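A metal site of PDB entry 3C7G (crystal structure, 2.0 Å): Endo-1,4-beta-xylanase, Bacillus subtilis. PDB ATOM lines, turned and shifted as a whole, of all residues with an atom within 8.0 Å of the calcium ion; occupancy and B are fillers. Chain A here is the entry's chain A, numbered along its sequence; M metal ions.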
ATOM      1  N   THR A  75      27.886  20.960 -17.638  1.00  0.00           N
ATOM      2  CA  THR A  75      26.807  20.306 -16.908  1.00  0.00           C
ATOM      3  C   THR A  75      27.314  20.012 -15.522  1.00  0.00           C
ATOM      4  O   THR A  75      28.349  19.363 -15.380  1.00  0.00           O
ATOM      5  CB  THR A  75      26.370  18.977 -17.581  1.00  0.00           C
ATOM      6  OG1 THR A  75      25.937  19.263 -18.900  1.00  0.00           O
ATOM      7  CG2 THR A  75      25.232  18.320 -16.793  1.00  0.00           C
ATOM      8  N   ASP A  76      26.589  20.477 -14.521  1.00  0.00           N
ATOM      9  CA  ASP A  76      26.997  20.172 -13.168  1.00  0.00           C
ATOM     10  C   ASP A  76      26.364  18.854 -12.756  1.00  0.00           C
ATOM     11  O   ASP A  76      25.137  18.749 -12.736  1.00  0.00           O
ATOM     12  CB  ASP A  76      26.624  21.292 -12.190  1.00  0.00           C
ATOM     13  CG  ASP A  76      27.496  21.253 -10.937  1.00  0.00           C
ATOM     14  OD1 ASP A  76      27.549  20.164 -10.322  1.00  0.00           O
ATOM     15  OD2 ASP A  76      28.142  22.265 -10.616  1.00  0.00           O
ATOM     16  N   ARG A 358      16.420  17.961 -24.426  1.00  0.00           N
ATOM     17  CA  ARG A 358      16.394  18.358 -23.050  1.00  0.00           C
ATOM     18  C   ARG A 358      17.826  18.765 -22.656  1.00  0.00           C
ATOM     19  O   ARG A 358      18.788  18.037 -22.901  1.00  0.00           O
ATOM     20  CB  ARG A 358      15.916  17.212 -22.169  1.00  0.00           C
ATOM     21  CG  ARG A 358      16.103  17.499 -20.697  1.00  0.00           C
ATOM     22  CD  ARG A 358      15.646  16.334 -19.831  1.00  0.00           C
ATOM     23  NE  ARG A 358      16.182  16.489 -18.484  1.00  0.00           N
ATOM     24  CZ  ARG A 358      15.564  16.090 -17.389  1.00  0.00           C
ATOM     25  NH1 ARG A 358      14.376  15.487 -17.481  1.00  0.00           N
ATOM     26  NH2 ARG A 358      16.128  16.302 -16.201  1.00  0.00           N
ATOM     27  N   VAL A 359      17.944  19.964 -22.099  1.00  0.00           N
ATOM     28  CA  VAL A 359      19.232  20.464 -21.620  1.00  0.00           C
ATOM     29  C   VAL A 359      19.007  20.765 -20.145  1.00  0.00           C
ATOM     30  O   VAL A 359      18.055  21.428 -19.785  1.00  0.00           O
ATOM     31  CB  VAL A 359      19.680  21.743 -22.381  1.00  0.00           C
ATOM     32  CG1 VAL A 359      20.976  22.314 -21.791  1.00  0.00           C
ATOM     33  CG2 VAL A 359      19.811  21.481 -23.903  1.00  0.00           C
ATOM     34  N   GLU A 360      19.874  20.219 -19.299  1.00  0.00           N
ATOM     35  CA  GLU A 360      19.777  20.485 -17.880  1.00  0.00           C
ATOM     36  C   GLU A 360      19.969  21.995 -17.652  1.00  0.00           C
ATOM     37  O   GLU A 360      20.791  22.616 -18.299  1.00  0.00           O
ATOM     38  CB  GLU A 360      20.854  19.690 -17.137  1.00  0.00           C
ATOM     39  CG  GLU A 360      20.676  18.171 -17.239  1.00  0.00           C
ATOM     40  CD  GLU A 360      19.247  17.713 -16.957  1.00  0.00           C
ATOM     41  OE1 GLU A 360      18.616  18.126 -15.956  1.00  0.00           O
ATOM     42  OE2 GLU A 360      18.739  16.934 -17.759  1.00  0.00           O
ATOM     43  N   ALA A 361      19.195  22.583 -16.750  1.00  0.00           N
ATOM     44  CA  ALA A 361      19.397  23.967 -16.385  1.00  0.00           C
ATOM     45  C   ALA A 361      20.841  24.181 -15.858  1.00  0.00           C
ATOM     46  O   ALA A 361      21.467  25.210 -16.097  1.00  0.00           O
ATOM     47  CB  ALA A 361      18.352  24.381 -15.344  1.00  0.00           C
ATOM     48  N   GLU A 362      21.351  23.163 -15.157  1.00  0.00           N
ATOM     49  CA  GLU A 362      22.693  23.168 -14.553  1.00  0.00           C
ATOM     50  C   GLU A 362      23.771  22.878 -15.589  1.00  0.00           C
ATOM     51  O   GLU A 362      24.922  22.592 -15.244  1.00  0.00           O
ATOM     52  CB  GLU A 362      22.760  22.104 -13.448  1.00  0.00           C
ATOM     53  CG  GLU A 362      22.595  20.648 -13.973  1.00  0.00           C
ATOM     54  CD  GLU A 362      21.153  20.096 -13.886  1.00  0.00           C
ATOM     55  OE1 GLU A 362      20.145  20.862 -13.920  1.00  0.00           O
ATOM     56  OE2 GLU A 362      21.015  18.856 -13.831  1.00  0.00           O
ATOM     57  N   THR A 363      23.386  22.933 -16.860  1.00  0.00           N
ATOM     58  CA  THR A 363      24.320  22.965 -17.985  1.00  0.00           C
ATOM     59  C   THR A 363      24.413  24.417 -18.447  1.00  0.00           C
ATOM     60  O   THR A 363      23.541  24.896 -19.169  1.00  0.00           O
ATOM     61  CB  THR A 363      23.843  22.076 -19.175  1.00  0.00           C
ATOM     62  OG1 THR A 363      23.804  20.717 -18.771  1.00  0.00           O
ATOM     63  CG2 THR A 363      24.779  22.229 -20.384  1.00  0.00           C
ATOM     64  N   GLU A 373      22.390  22.269  -6.961  1.00  0.00           N
ATOM     65  CA  GLU A 373      22.235  21.249  -5.891  1.00  0.00           C
ATOM     66  C   GLU A 373      21.568  20.089  -6.629  1.00  0.00           C
ATOM     67  O   GLU A 373      20.790  20.323  -7.548  1.00  0.00           O
ATOM     68  CB  GLU A 373      21.492  21.794  -4.692  1.00  0.00           C
ATOM     69  CG  GLU A 373      20.038  21.950  -4.907  1.00  0.00           C
ATOM     70  CD  GLU A 373      19.350  22.608  -3.737  1.00  0.00           C
ATOM     71  OE1 GLU A 373      20.021  22.821  -2.699  1.00  0.00           O
ATOM     72  OE2 GLU A 373      18.149  22.917  -3.887  1.00  0.00           O
ATOM     73  N   LYS A 374      21.745  18.830  -6.235  1.00  0.00           N
ATOM     74  CA  LYS A 374      20.696  17.866  -5.965  1.00  0.00           C
ATOM     75  C   LYS A 374      19.226  18.209  -6.071  1.00  0.00           C
ATOM     76  O   LYS A 374      18.694  18.910  -5.236  1.00  0.00           O
ATOM     77  CB  LYS A 374      21.056  16.746  -4.994  1.00  0.00           C
ATOM     78  CG  LYS A 374      20.536  15.389  -5.492  1.00  0.00           C
ATOM     79  CD  LYS A 374      21.283  14.239  -4.787  1.00  0.00           C
ATOM     80  CE  LYS A 374      20.516  12.940  -4.774  1.00  0.00           C
ATOM     81  NZ  LYS A 374      19.881  12.589  -6.082  1.00  0.00           N
ATOM     82  N   SER A 375      18.584  17.683  -7.124  1.00  0.00           N
ATOM     83  CA  SER A 375      17.191  18.004  -7.392  1.00  0.00           C
ATOM     84  C   SER A 375      16.176  16.945  -6.972  1.00  0.00           C
ATOM     85  O   SER A 375      16.427  15.748  -7.092  1.00  0.00           O
ATOM     86  CB  SER A 375      16.976  18.259  -8.874  1.00  0.00           C
ATOM     87  OG  SER A 375      15.709  18.836  -9.061  1.00  0.00           O
ATOM     88  N   ALA A 377      13.407  16.754  -8.679  1.00  0.00           N
ATOM     89  CA  ALA A 377      12.568  16.638  -9.867  1.00  0.00           C
ATOM     90  C   ALA A 377      12.452  15.169 -10.243  1.00  0.00           C
ATOM     91  O   ALA A 377      13.468  14.467 -10.261  1.00  0.00           O
ATOM     92  CB  ALA A 377      13.133  17.440 -11.002  1.00  0.00           C
ATOM     93  N   GLY A 379      12.354  11.892 -12.471  1.00  0.00           N
ATOM     94  CA  GLY A 379      13.106  11.520 -13.672  1.00  0.00           C
ATOM     95  C   GLY A 379      14.441  12.252 -13.713  1.00  0.00           C
ATOM     96  O   GLY A 379      15.006  12.628 -12.668  1.00  0.00           O
ATOM     97  N   GLY A 380      14.943  12.482 -14.921  1.00  0.00           N
ATOM     98  CA  GLY A 380      16.210  13.174 -15.089  1.00  0.00           C
ATOM     99  C   GLY A 380      17.400  12.217 -15.066  1.00  0.00           C
ATOM    100  O   GLY A 380      17.248  11.027 -14.791  1.00  0.00           O
ATOM    101  N   PRO A 381      18.600  12.742 -15.342  1.00  0.00           N
ATOM    102  CA  PRO A 381      19.795  11.940 -15.412  1.00  0.00           C
ATOM    103  C   PRO A 381      20.250  11.544 -14.024  1.00  0.00           C
ATOM    104  O   PRO A 381      19.672  11.992 -13.027  1.00  0.00           O
ATOM    105  CB  PRO A 381      20.825  12.883 -16.054  1.00  0.00           C
ATOM    106  CG  PRO A 381      20.363  14.228 -15.716  1.00  0.00           C
ATOM    107  CD  PRO A 381      18.861  14.174 -15.638  1.00  0.00           C
ATOM    108  N   ASN A 383      21.993  11.562 -10.643  1.00  0.00           N
ATOM    109  CA  ASN A 383      22.355  12.652  -9.753  1.00  0.00           C
ATOM    110  C   ASN A 383      21.851  13.989 -10.296  1.00  0.00           C
ATOM    111  O   ASN A 383      22.523  15.014 -10.181  1.00  0.00           O
ATOM    112  CB  ASN A 383      23.874  12.694  -9.494  1.00  0.00           C
ATOM    113  CG  ASN A 383      24.211  13.179  -8.098  1.00  0.00           C
ATOM    114  OD1 ASN A 383      23.494  12.867  -7.140  1.00  0.00           O
ATOM    115  ND2 ASN A 383      25.293  13.962  -7.961  1.00  0.00           N
ATOM    116  N   ASN A 384      20.670  13.943 -10.923  1.00  0.00           N
ATOM    117  CA  ASN A 384      20.069  15.148 -11.457  1.00  0.00           C
ATOM    118  C   ASN A 384      20.152  16.349 -10.487  1.00  0.00           C
ATOM    119  O   ASN A 384      19.814  16.258  -9.301  1.00  0.00           O
ATOM    120  CB  ASN A 384      18.622  14.883 -11.865  1.00  0.00           C
ATOM    121  CG  ASN A 384      17.991  16.085 -12.531  1.00  0.00           C
ATOM    122  OD1 ASN A 384      18.626  16.735 -13.343  1.00  0.00           O
ATOM    123  ND2 ASN A 384      16.772  16.398 -12.169  1.00  0.00           N
ATOM    124  N   GLN A 385      20.637  17.468 -11.004  1.00  0.00           N
ATOM    125  CA  GLN A 385      20.754  18.688 -10.237  1.00  0.00           C
ATOM    126  C   GLN A 385      19.680  19.669 -10.700  1.00  0.00           C
ATOM    127  O   GLN A 385      18.948  19.441 -11.685  1.00  0.00           O
ATOM    128  CB  GLN A 385      22.145  19.323 -10.436  1.00  0.00           C
ATOM    129  CG  GLN A 385      23.309  18.399 -10.127  1.00  0.00           C
ATOM    130  CD  GLN A 385      23.537  18.210  -8.641  1.00  0.00           C
ATOM    131  OE1 GLN A 385      23.860  19.168  -7.940  1.00  0.00           O
ATOM    132  NE2 GLN A 385      23.371  16.989  -8.155  1.00  0.00           N
ATOM    133  N   HIS A 386      19.562  20.777  -9.992  1.00  0.00           N
ATOM    134  CA  HIS A 386      18.855  21.909 -10.551  1.00  0.00           C
ATOM    135  C   HIS A 386      19.608  23.182 -10.181  1.00  0.00           C
ATOM    136  O   HIS A 386      20.510  23.174  -9.330  1.00  0.00           O
ATOM    137  CB  HIS A 386      17.392  21.945 -10.085  1.00  0.00           C
ATOM    138  CG  HIS A 386      17.221  21.990  -8.602  1.00  0.00           C
ATOM    139  ND1 HIS A 386      16.234  21.277  -7.960  1.00  0.00           N
ATOM    140  CD2 HIS A 386      17.883  22.670  -7.642  1.00  0.00           C
ATOM    141  CE1 HIS A 386      16.304  21.510  -6.667  1.00  0.00           C
ATOM    142  NE2 HIS A 386      17.282  22.368  -6.447  1.00  0.00           N
ATOM    143  N   VAL A 387      19.252  24.265 -10.866  1.00  0.00           N
ATOM    144  CA  VAL A 387      19.749  25.592 -10.530  1.00  0.00           C
ATOM    145  C   VAL A 387      18.857  26.156  -9.433  1.00  0.00           C
ATOM    146  O   VAL A 387      17.618  26.106  -9.501  1.00  0.00           O
ATOM    147  CB  VAL A 387      19.762  26.527 -11.750  1.00  0.00           C
ATOM    148  CG1 VAL A 387      20.158  27.973 -11.326  1.00  0.00           C
ATOM    149  CG2 VAL A 387      20.747  25.995 -12.807  1.00  0.00           C
ATOM    150  N   ASN A 414      11.394  22.941 -16.773  1.00  0.00           N
ATOM    151  CA  ASN A 414      10.884  22.201 -15.632  1.00  0.00           C
ATOM    152  C   ASN A 414      11.281  22.945 -14.383  1.00  0.00           C
ATOM    153  O   ASN A 414      12.474  23.148 -14.125  1.00  0.00           O
ATOM    154  CB  ASN A 414      11.436  20.774 -15.639  1.00  0.00           C
ATOM    155  CG  ASN A 414      10.604  19.845 -14.806  1.00  0.00           C
ATOM    156  OD1 ASN A 414       9.382  19.901 -14.856  1.00  0.00           O
ATOM    157  ND2 ASN A 414      11.258  18.954 -14.048  1.00  0.00           N
ATOM    158  N   TRP A 449       7.080  19.850  -9.227  1.00  0.00           N
ATOM    159  CA  TRP A 449       7.664  20.161 -10.505  1.00  0.00           C
ATOM    160  C   TRP A 449       6.608  20.218 -11.586  1.00  0.00           C
ATOM    161  O   TRP A 449       5.743  19.344 -11.684  1.00  0.00           O
ATOM    162  CB  TRP A 449       8.719  19.096 -10.820  1.00  0.00           C
ATOM    163  CG  TRP A 449       9.854  19.271  -9.874  1.00  0.00           C
ATOM    164  CD1 TRP A 449       9.987  18.688  -8.655  1.00  0.00           C
ATOM    165  CD2 TRP A 449      10.953  20.165 -10.026  1.00  0.00           C
ATOM    166  NE1 TRP A 449      11.121  19.146  -8.033  1.00  0.00           N
ATOM    167  CE2 TRP A 449      11.744  20.048  -8.851  1.00  0.00           C
ATOM    168  CE3 TRP A 449      11.357  21.058 -11.025  1.00  0.00           C
ATOM    169  CZ2 TRP A 449      12.931  20.774  -8.662  1.00  0.00           C
ATOM    170  CZ3 TRP A 449      12.538  21.792 -10.834  1.00  0.00           C
ATOM    171  CH2 TRP A 449      13.310  21.633  -9.665  1.00  0.00           C
ATOM    172  N   PHE A 480      14.932  24.949 -11.079  1.00  0.00           N
ATOM    173  CA  PHE A 480      15.098  25.218 -12.471  1.00  0.00           C
ATOM    174  C   PHE A 480      15.924  23.973 -12.784  1.00  0.00           C
ATOM    175  O   PHE A 480      17.130  23.927 -12.529  1.00  0.00           O
ATOM    176  CB  PHE A 480      15.740  26.529 -12.927  1.00  0.00           C
ATOM    177  CG  PHE A 480      15.751  26.673 -14.420  1.00  0.00           C
ATOM    178  CD1 PHE A 480      15.007  25.795 -15.234  1.00  0.00           C
ATOM    179  CD2 PHE A 480      16.500  27.675 -15.042  1.00  0.00           C
ATOM    180  CE1 PHE A 480      15.025  25.911 -16.651  1.00  0.00           C
ATOM    181  CE2 PHE A 480      16.513  27.818 -16.429  1.00  0.00           C
ATOM    182  CZ  PHE A 480      15.788  26.918 -17.249  1.00  0.00           C
ATOM    183  N   ASP A 481      15.222  22.948 -13.285  1.00  0.00           N
ATOM    184  CA  ASP A 481      15.782  21.596 -13.478  1.00  0.00           C
ATOM    185  C   ASP A 481      16.309  21.361 -14.904  1.00  0.00           C
ATOM    186  O   ASP A 481      17.398  20.884 -15.101  1.00  0.00           O
ATOM    187  CB  ASP A 481      14.685  20.545 -13.105  1.00  0.00           C
ATOM    188  CG  ASP A 481      15.066  19.091 -13.456  1.00  0.00           C
ATOM    189  OD1 ASP A 481      16.262  18.696 -13.359  1.00  0.00           O
ATOM    190  OD2 ASP A 481      14.128  18.306 -13.763  1.00  0.00           O
ATOM    191  N   TYR A 482      15.498  21.656 -15.900  1.00  0.00           N
ATOM    192  CA  TYR A 482      15.903  21.448 -17.272  1.00  0.00           C
ATOM    193  C   TYR A 482      15.025  22.330 -18.127  1.00  0.00           C
ATOM    194  O   TYR A 482      14.029  22.872 -17.675  1.00  0.00           O
ATOM    195  CB  TYR A 482      15.782  19.967 -17.718  1.00  0.00           C
ATOM    196  CG  TYR A 482      14.352  19.457 -17.935  1.00  0.00           C
ATOM    197  CD1 TYR A 482      13.669  19.716 -19.125  1.00  0.00           C
ATOM    198  CD2 TYR A 482      13.735  18.685 -16.974  1.00  0.00           C
ATOM    199  CE1 TYR A 482      12.370  19.251 -19.326  1.00  0.00           C
ATOM    200  CE2 TYR A 482      12.455  18.195 -17.172  1.00  0.00           C
ATOM    201  CZ  TYR A 482      11.788  18.488 -18.337  1.00  0.00           C
ATOM    202  OH  TYR A 482      10.500  18.009 -18.500  1.00  0.00           O
ATOM    203  N   TRP A 483      15.464  22.482 -19.357  1.00  0.00           N
ATOM    204  CA  TRP A 483      14.714  23.213 -20.341  1.00  0.00           C
ATOM    205  C   TRP A 483      14.901  22.509 -21.675  1.00  0.00           C
ATOM    206  O   TRP A 483      15.799  21.662 -21.851  1.00  0.00           O
ATOM    207  CB  TRP A 483      15.158  24.693 -20.370  1.00  0.00           C
ATOM    208  CG  TRP A 483      16.652  24.925 -20.524  1.00  0.00           C
ATOM    209  CD1 TRP A 483      17.548  25.171 -19.518  1.00  0.00           C
ATOM    210  CD2 TRP A 483      17.390  24.943 -21.734  1.00  0.00           C
ATOM    211  NE1 TRP A 483      18.806  25.349 -20.032  1.00  0.00           N
ATOM    212  CE2 TRP A 483      18.749  25.216 -21.395  1.00  0.00           C
ATOM    213  CE3 TRP A 483      17.052  24.776 -23.091  1.00  0.00           C
ATOM    214  CZ2 TRP A 483      19.767  25.320 -22.359  1.00  0.00           C
ATOM    215  CZ3 TRP A 483      18.061  24.866 -24.039  1.00  0.00           C
ATOM    216  CH2 TRP A 483      19.397  25.139 -23.670  1.00  0.00           C
HETATM  217 CA    CA M   1      18.541  19.031 -13.954  1.00  0.00          CA
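OE1 of Gln 385 sits close to O of Glu 373.
The backbone carbonyl oxygen (O) of Asn 384 is in hydrogen-bond range of the backbone NH (N) of Ser 375 (2.9 Å).
The backbone NH (N) of Asp 481 is in hydrogen-bond range of the backbone carbonyl oxygen (O) of Asn 414, 2.9 Å away.
OE1 of Gln 385 lies within hydrogen-bond range of N of Lys 374, 2.7 Å away.
OE2 of Glu 360 lies within salt-bridge range of NE of Arg 358 (2.7 Å).
The backbone carbonyl oxygen (O) of Asn 383 lies within hydrogen-bond range of the side-chain amide nitrogen (NE2) of Gln 385 (3.0 Å).
The backbone carbonyl oxygen of Glu 362 is in hydrogen-bond range of the backbone NH of Asp 76, at 2.8 Å.
The side-chain carboxylate (OD2) of Asp 481 is in salt-bridge range of the guanidinium group (NH2) of Arg 358, at 3.7 Å.
The calcium ion is bound by the side-chain carboxylate (OE1) of Glu 360 (2.2 Å), the backbone carbonyl oxygen (O) of Gln 385 (2.3 Å), the side-chain amide oxygen (OD1) of Asn 384 (2.4 Å), the side-chain carboxylate (OD1) of Asp 481 (2.4 Å), the side-chain carboxylate (OE1) of Glu 362 (2.4 Å), the backbone carbonyl oxygen (O) of Asp 481 (2.5 Å) and the side-chain carboxylate (OE2) of Glu 362 (2.5 Å).
Within 4 Å of the calcium ion: Glu 360, Glu 362, Asn 384, Gln 385 and Asp 481.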
